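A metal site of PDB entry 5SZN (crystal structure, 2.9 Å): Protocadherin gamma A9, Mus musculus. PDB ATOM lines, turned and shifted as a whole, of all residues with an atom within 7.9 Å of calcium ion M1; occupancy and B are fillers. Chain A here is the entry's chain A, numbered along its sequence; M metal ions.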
ATOM      1  N   ASP A  97     -10.758  26.266   5.732  1.00  0.00           N
ATOM      2  CA  ASP A  97     -12.208  26.223   5.715  1.00  0.00           C
ATOM      3  C   ASP A  97     -12.780  27.298   6.624  1.00  0.00           C
ATOM      4  O   ASP A  97     -12.303  27.500   7.747  1.00  0.00           O
ATOM      5  CB  ASP A  97     -12.725  24.850   6.141  1.00  0.00           C
ATOM      6  CG  ASP A  97     -14.236  24.730   6.031  1.00  0.00           C
ATOM      7  OD1 ASP A  97     -14.720  24.352   4.937  1.00  0.00           O
ATOM      8  OD2 ASP A  97     -14.941  25.010   7.021  1.00  0.00           O
ATOM      9  N   ILE A  98     -13.799  27.993   6.121  1.00  0.00           N
ATOM     10  CA  ILE A  98     -14.578  28.938   6.911  1.00  0.00           C
ATOM     11  C   ILE A  98     -16.023  28.449   6.941  1.00  0.00           C
ATOM     12  O   ILE A  98     -16.461  27.694   6.067  1.00  0.00           O
ATOM     13  CB  ILE A  98     -14.495  30.377   6.373  1.00  0.00           C
ATOM     14  CG1 ILE A  98     -15.259  30.503   5.050  1.00  0.00           C
ATOM     15  CG2 ILE A  98     -13.036  30.795   6.196  1.00  0.00           C
ATOM     16  CD1 ILE A  98     -15.134  31.856   4.395  1.00  0.00           C
ATOM     17  N   ASN A  99     -16.750  28.888   7.960  1.00  0.00           N
ATOM     18  CA  ASN A  99     -18.132  28.451   8.160  1.00  0.00           C
ATOM     19  C   ASN A  99     -19.062  29.398   7.417  1.00  0.00           C
ATOM     20  O   ASN A  99     -19.458  30.448   7.937  1.00  0.00           O
ATOM     21  CB  ASN A  99     -18.477  28.368   9.637  1.00  0.00           C
ATOM     22  CG  ASN A  99     -19.874  27.827   9.877  1.00  0.00           C
ATOM     23  OD1 ASN A  99     -20.357  26.982   9.125  1.00  0.00           O
ATOM     24  ND2 ASN A  99     -20.529  28.326  10.917  1.00  0.00           N
ATOM     25  N   ASP A 100     -19.421  29.039   6.189  1.00  0.00           N
ATOM     26  CA  ASP A 100     -20.404  29.769   5.420  1.00  0.00           C
ATOM     27  C   ASP A 100     -21.641  28.955   5.077  1.00  0.00           C
ATOM     28  O   ASP A 100     -22.687  29.540   4.787  1.00  0.00           O
ATOM     29  CB  ASP A 100     -19.783  30.291   4.104  1.00  0.00           C
ATOM     30  CG  ASP A 100     -19.181  29.181   3.273  1.00  0.00           C
ATOM     31  OD1 ASP A 100     -18.567  28.268   3.855  1.00  0.00           O
ATOM     32  OD2 ASP A 100     -19.333  29.203   2.033  1.00  0.00           O
ATOM     33  N   ASN A 101     -21.551  27.627   5.094  1.00  0.00           N
ATOM     34  CA  ASN A 101     -22.659  26.751   4.730  1.00  0.00           C
ATOM     35  C   ASN A 101     -23.404  26.315   5.984  1.00  0.00           C
ATOM     36  O   ASN A 101     -22.798  25.983   7.007  1.00  0.00           O
ATOM     37  CB  ASN A 101     -22.150  25.518   3.978  1.00  0.00           C
ATOM     38  CG  ASN A 101     -21.765  25.834   2.540  1.00  0.00           C
ATOM     39  OD1 ASN A 101     -21.813  24.961   1.671  1.00  0.00           O
ATOM     40  ND2 ASN A 101     -21.392  27.077   2.284  1.00  0.00           N
ATOM     41  N   ALA A 102     -24.728  26.329   5.901  1.00  0.00           N
ATOM     42  CA  ALA A 102     -25.565  25.815   6.974  1.00  0.00           C
ATOM     43  C   ALA A 102     -25.897  24.341   6.748  1.00  0.00           C
ATOM     44  O   ALA A 102     -25.964  23.897   5.594  1.00  0.00           O
ATOM     45  CB  ALA A 102     -26.855  26.623   7.079  1.00  0.00           C
ATOM     46  N   PRO A 103     -26.082  23.565   7.807  1.00  0.00           N
ATOM     47  CA  PRO A 103     -26.470  22.162   7.629  1.00  0.00           C
ATOM     48  C   PRO A 103     -27.823  22.059   6.940  1.00  0.00           C
ATOM     49  O   PRO A 103     -28.663  22.950   7.027  1.00  0.00           O
ATOM     50  CB  PRO A 103     -26.518  21.611   9.050  1.00  0.00           C
ATOM     51  CG  PRO A 103     -26.663  22.812   9.926  1.00  0.00           C
ATOM     52  CD  PRO A 103     -25.910  23.912   9.232  1.00  0.00           C
ATOM     53  N   LYS A 104     -28.021  20.943   6.222  1.00  0.00           N
ATOM     54  CA  LYS A 104     -29.220  20.731   5.443  1.00  0.00           C
ATOM     55  C   LYS A 104     -29.798  19.357   5.710  1.00  0.00           C
ATOM     56  O   LYS A 104     -29.063  18.391   5.966  1.00  0.00           O
ATOM     57  CB  LYS A 104     -28.936  20.883   3.940  1.00  0.00           C
ATOM     58  N   VAL A 130     -26.665  17.173   7.037  1.00  0.00           N
ATOM     59  CA  VAL A 130     -25.350  17.178   6.417  1.00  0.00           C
ATOM     60  C   VAL A 130     -24.862  18.616   6.294  1.00  0.00           C
ATOM     61  O   VAL A 130     -25.643  19.519   5.971  1.00  0.00           O
ATOM     62  CB  VAL A 130     -25.368  16.486   5.033  1.00  0.00           C
ATOM     63  CG1 VAL A 130     -25.420  14.977   5.186  1.00  0.00           C
ATOM     64  CG2 VAL A 130     -26.553  16.981   4.207  1.00  0.00           C
ATOM     65  N   ASP A 131     -23.570  18.826   6.557  1.00  0.00           N
ATOM     66  CA  ASP A 131     -22.966  20.143   6.493  1.00  0.00           C
ATOM     67  C   ASP A 131     -21.753  20.058   5.571  1.00  0.00           C
ATOM     68  O   ASP A 131     -20.826  19.261   5.841  1.00  0.00           O
ATOM     69  CB  ASP A 131     -22.566  20.633   7.886  1.00  0.00           C
ATOM     70  CG  ASP A 131     -22.062  22.068   7.878  1.00  0.00           C
ATOM     71  OD1 ASP A 131     -22.286  22.782   6.887  1.00  0.00           O
ATOM     72  OD2 ASP A 131     -21.456  22.489   8.890  1.00  0.00           O
ATOM     73  N   PRO A 132     -21.715  20.831   4.480  1.00  0.00           N
ATOM     74  CA  PRO A 132     -20.572  20.737   3.547  1.00  0.00           C
ATOM     75  C   PRO A 132     -19.226  21.064   4.173  1.00  0.00           C
ATOM     76  O   PRO A 132     -18.205  20.608   3.659  1.00  0.00           O
ATOM     77  CB  PRO A 132     -20.938  21.741   2.450  1.00  0.00           C
ATOM     78  CG  PRO A 132     -22.420  21.846   2.510  1.00  0.00           C
ATOM     79  CD  PRO A 132     -22.788  21.699   3.958  1.00  0.00           C
ATOM     80  N   ASP A 133     -19.195  21.827   5.265  1.00  0.00           N
ATOM     81  CA  ASP A 133     -17.941  22.226   5.876  1.00  0.00           C
ATOM     82  C   ASP A 133     -17.271  21.028   6.549  1.00  0.00           C
ATOM     83  O   ASP A 133     -17.806  19.918   6.612  1.00  0.00           O
ATOM     84  CB  ASP A 133     -18.176  23.362   6.869  1.00  0.00           C
ATOM     85  CG  ASP A 133     -18.815  24.573   6.225  1.00  0.00           C
ATOM     86  OD1 ASP A 133     -18.506  24.857   5.053  1.00  0.00           O
ATOM     87  OD2 ASP A 133     -19.645  25.239   6.886  1.00  0.00           O
ATOM     88  N   VAL A 134     -16.054  21.262   7.060  1.00  0.00           N
ATOM     89  CA  VAL A 134     -15.238  20.220   7.673  1.00  0.00           C
ATOM     90  C   VAL A 134     -14.690  20.737   8.998  1.00  0.00           C
ATOM     91  O   VAL A 134     -14.319  21.911   9.103  1.00  0.00           O
ATOM     92  CB  VAL A 134     -14.085  19.784   6.737  1.00  0.00           C
ATOM     93  CG1 VAL A 134     -13.179  18.780   7.421  1.00  0.00           C
ATOM     94  CG2 VAL A 134     -14.630  19.217   5.436  1.00  0.00           C
ATOM     95  N   GLY A 135     -14.649  19.861   9.996  1.00  0.00           N
ATOM     96  CA  GLY A 135     -14.084  20.213  11.288  1.00  0.00           C
ATOM     97  C   GLY A 135     -15.070  20.917  12.186  1.00  0.00           C
ATOM     98  O   GLY A 135     -16.227  20.493  12.310  1.00  0.00           O
ATOM     99  N   ILE A 136     -14.624  21.989  12.844  1.00  0.00           N
ATOM    100  CA  ILE A 136     -15.513  22.748  13.719  1.00  0.00           C
ATOM    101  C   ILE A 136     -16.640  23.381  12.920  1.00  0.00           C
ATOM    102  O   ILE A 136     -17.780  23.483  13.389  1.00  0.00           O
ATOM    103  CB  ILE A 136     -14.717  23.803  14.514  1.00  0.00           C
ATOM    104  CG1 ILE A 136     -13.585  23.133  15.295  1.00  0.00           C
ATOM    105  CG2 ILE A 136     -15.622  24.574  15.455  1.00  0.00           C
ATOM    106  CD1 ILE A 136     -14.063  22.103  16.308  1.00  0.00           C
ATOM    107  N   ASN A 137     -16.340  23.813  11.692  1.00  0.00           N
ATOM    108  CA  ASN A 137     -17.360  24.444  10.857  1.00  0.00           C
ATOM    109  C   ASN A 137     -18.426  23.454  10.395  1.00  0.00           C
ATOM    110  O   ASN A 137     -19.496  23.892   9.944  1.00  0.00           O
ATOM    111  CB  ASN A 137     -16.705  25.102   9.642  1.00  0.00           C
ATOM    112  CG  ASN A 137     -15.650  26.119  10.035  1.00  0.00           C
ATOM    113  OD1 ASN A 137     -15.704  26.718  11.107  1.00  0.00           O
ATOM    114  ND2 ASN A 137     -14.669  26.325   9.157  1.00  0.00           N
ATOM    115  N   SER A 138     -18.160  22.158  10.498  1.00  0.00           N
ATOM    116  CA  SER A 138     -19.148  21.158  10.127  1.00  0.00           C
ATOM    117  C   SER A 138     -20.183  20.996  11.242  1.00  0.00           C
ATOM    118  O   SER A 138     -20.170  21.714  12.251  1.00  0.00           O
ATOM    119  CB  SER A 138     -18.474  19.824   9.819  1.00  0.00           C
ATOM    120  OG  SER A 138     -19.422  18.855   9.399  1.00  0.00           O
ATOM    121  N   LEU A 139     -21.100  20.041  11.064  1.00  0.00           N
ATOM    122  CA  LEU A 139     -22.171  19.825  12.023  1.00  0.00           C
ATOM    123  C   LEU A 139     -21.607  19.469  13.388  1.00  0.00           C
ATOM    124  O   LEU A 139     -20.640  18.712  13.509  1.00  0.00           O
ATOM    125  CB  LEU A 139     -23.095  18.708  11.533  1.00  0.00           C
ATOM    126  CG  LEU A 139     -24.279  18.335  12.428  1.00  0.00           C
ATOM    127  CD1 LEU A 139     -25.375  19.374  12.328  1.00  0.00           C
ATOM    128  CD2 LEU A 139     -24.792  16.950  12.097  1.00  0.00           C
ATOM    129  N   GLN A 140     -22.218  20.028  14.436  1.00  0.00           N
ATOM    130  CA  GLN A 140     -21.814  19.743  15.804  1.00  0.00           C
ATOM    131  C   GLN A 140     -22.892  19.045  16.620  1.00  0.00           C
ATOM    132  O   GLN A 140     -22.634  17.969  17.181  1.00  0.00           O
ATOM    133  CB  GLN A 140     -21.376  21.024  16.527  1.00  0.00           C
ATOM    134  CG  GLN A 140     -20.940  20.767  17.965  1.00  0.00           C
ATOM    135  CD  GLN A 140     -20.615  22.038  18.732  1.00  0.00           C
ATOM    136  OE1 GLN A 140     -20.442  23.099  18.148  1.00  0.00           O
ATOM    137  NE2 GLN A 140     -20.537  21.920  20.053  1.00  0.00           N
ATOM    138  N   TYR A 187     -27.166  22.293  14.565  1.00  0.00           N
ATOM    139  CA  TYR A 187     -26.178  23.318  14.876  1.00  0.00           C
ATOM    140  C   TYR A 187     -24.780  22.864  14.466  1.00  0.00           C
ATOM    141  O   TYR A 187     -24.423  21.691  14.642  1.00  0.00           O
ATOM    142  CB  TYR A 187     -26.140  23.658  16.367  1.00  0.00           C
ATOM    143  CG  TYR A 187     -27.397  24.278  16.923  1.00  0.00           C
ATOM    144  CD1 TYR A 187     -27.741  25.593  16.628  1.00  0.00           C
ATOM    145  CD2 TYR A 187     -28.230  23.561  17.772  1.00  0.00           C
ATOM    146  CE1 TYR A 187     -28.889  26.166  17.143  1.00  0.00           C
ATOM    147  CE2 TYR A 187     -29.369  24.119  18.298  1.00  0.00           C
ATOM    148  CZ  TYR A 187     -29.697  25.425  17.977  1.00  0.00           C
ATOM    149  OH  TYR A 187     -30.835  25.998  18.502  1.00  0.00           O
ATOM    150  N   ASP A 188     -23.994  23.798  13.953  1.00  0.00           N
ATOM    151  CA  ASP A 188     -22.573  23.626  13.700  1.00  0.00           C
ATOM    152  C   ASP A 188     -21.771  24.415  14.731  1.00  0.00           C
ATOM    153  O   ASP A 188     -22.323  25.157  15.546  1.00  0.00           O
ATOM    154  CB  ASP A 188     -22.216  24.059  12.275  1.00  0.00           C
ATOM    155  CG  ASP A 188     -22.517  25.528  12.003  1.00  0.00           C
ATOM    156  OD1 ASP A 188     -23.191  26.168  12.837  1.00  0.00           O
ATOM    157  OD2 ASP A 188     -22.089  26.028  10.950  1.00  0.00           O
ATOM    158  N   GLY A 189     -20.451  24.239  14.690  1.00  0.00           N
ATOM    159  CA  GLY A 189     -19.596  24.838  15.700  1.00  0.00           C
ATOM    160  C   GLY A 189     -18.892  26.117  15.274  1.00  0.00           C
ATOM    161  O   GLY A 189     -18.370  26.849  16.121  1.00  0.00           O
ATOM    162  N   GLY A 190     -18.868  26.398  13.976  1.00  0.00           N
ATOM    163  CA  GLY A 190     -18.161  27.553  13.471  1.00  0.00           C
ATOM    164  C   GLY A 190     -18.893  28.865  13.667  1.00  0.00           C
ATOM    165  O   GLY A 190     -19.687  29.277  12.816  1.00  0.00           O
ATOM    166  N   PRO A 192     -19.579  32.768  13.568  1.00  0.00           N
ATOM    167  CA  PRO A 192     -21.040  32.838  13.696  1.00  0.00           C
ATOM    168  C   PRO A 192     -21.765  31.572  13.252  1.00  0.00           C
ATOM    169  O   PRO A 192     -21.700  31.195  12.078  1.00  0.00           O
ATOM    170  CB  PRO A 192     -21.421  34.023  12.801  1.00  0.00           C
ATOM    171  CG  PRO A 192     -20.182  34.847  12.722  1.00  0.00           C
ATOM    172  CD  PRO A 192     -19.058  33.858  12.716  1.00  0.00           C
ATOM    173  N   ARG A 193     -22.438  30.924  14.194  1.00  0.00           N
ATOM    174  CA  ARG A 193     -22.951  29.572  13.984  1.00  0.00           C
ATOM    175  C   ARG A 193     -24.195  29.588  13.119  1.00  0.00           C
ATOM    176  O   ARG A 193     -25.117  30.385  13.335  1.00  0.00           O
ATOM    177  CB  ARG A 193     -23.270  28.927  15.333  1.00  0.00           C
ATOM    178  CG  ARG A 193     -22.162  29.030  16.359  1.00  0.00           C
ATOM    179  CD  ARG A 193     -22.619  28.474  17.700  1.00  0.00           C
ATOM    180  NE  ARG A 193     -22.944  27.055  17.601  1.00  0.00           N
ATOM    181  CZ  ARG A 193     -23.731  26.412  18.457  1.00  0.00           C
ATOM    182  NH1 ARG A 193     -24.299  27.065  19.465  1.00  0.00           N
ATOM    183  NH2 ARG A 193     -23.968  25.118  18.303  1.00  0.00           N
ATOM    184  N   ARG A 194     -24.222  28.701  12.118  1.00  0.00           N
ATOM    185  CA  ARG A 194     -25.408  28.473  11.326  1.00  0.00           C
ATOM    186  C   ARG A 194     -26.304  27.442  12.025  1.00  0.00           C
ATOM    187  O   ARG A 194     -25.945  26.861  13.046  1.00  0.00           O
ATOM    188  CB  ARG A 194     -25.034  28.017   9.918  1.00  0.00           C
ATOM    189  CG  ARG A 194     -23.993  28.873   9.215  1.00  0.00           C
ATOM    190  CD  ARG A 194     -24.408  30.340   9.169  1.00  0.00           C
ATOM    191  NE  ARG A 194     -23.586  31.110   8.232  1.00  0.00           N
ATOM    192  CZ  ARG A 194     -22.376  31.583   8.508  1.00  0.00           C
ATOM    193  NH1 ARG A 194     -21.837  31.364   9.704  1.00  0.00           N
ATOM    194  NH2 ARG A 194     -21.699  32.267   7.594  1.00  0.00           N
ATOM    195  N   SER A 195     -27.482  27.203  11.455  1.00  0.00           N
ATOM    196  CA  SER A 195     -28.437  26.285  12.039  1.00  0.00           C
ATOM    197  C   SER A 195     -29.490  25.944  10.998  1.00  0.00           C
ATOM    198  O   SER A 195     -29.613  26.611   9.973  1.00  0.00           O
ATOM    199  CB  SER A 195     -29.097  26.879  13.288  1.00  0.00           C
ATOM    200  OG  SER A 195     -29.541  28.204  13.034  1.00  0.00           O
HETATM  201 CA    CA M   1     -21.769  24.701   8.851  1.00  0.00          CA
HETATM  202 CA    CA M   2     -16.887  26.598   3.794  1.00  0.00          CA
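The guanidinium group of Arg 194 is in hydrogen-bond range of the backbone carbonyl oxygen of Asn 99 (2.9 Å). The backbone carbonyl oxygen of Asp 133 sits close to the side-chain hydroxyl of Ser 138. ND2 of Asn 137 sits at hydrogen-bond distance from OD2 of Asp 97 (2.5 Å). The side-chain carboxylate (OD2) of Asp 133 sits close to the side-chain amide oxygen (OD1) of Asn 99 (2.9 Å). The side-chain amide nitrogen (ND2) of Asn 99 lies within hydrogen-bond range of the backbone carbonyl oxygen (O) of Pro 192, at 3.3 Å. The side-chain carboxylate (OD1) of Asp 188 lies within hydrogen-bond range of the backbone NH (N) of Arg 194, at 2.8 Å. O of Asp 188 sits at hydrogen-bond distance from NE of Arg 193 (2.9 Å). The side-chain carboxylate of Asp 131 lies close to the backbone NH of Leu 139, 3.3 Å away.
Of the 27 residues printed, 6 come within 4 Å of calcium ion M1.
Calcium ion M1 is bound by the side-chain carboxylate (OD2) of Asp 131 (2.2 Å), the backbone carbonyl oxygen (O) of Asn 101 (2.5 Å), the side-chain carboxylate (OD2) of Asp 188 (2.5 Å), the backbone carbonyl oxygen (O) of Asn 137 (2.6 Å), the side-chain amide oxygen (OD1) of Asn 99 (2.7 Å) and the side-chain carboxylate (OD1) of Asp 131 (2.8 Å). Calcium ion M1 has six donor atoms within binding distance. Slightly farther from calcium ion M1 lies OD2 of Asp 133 (2.9 Å).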
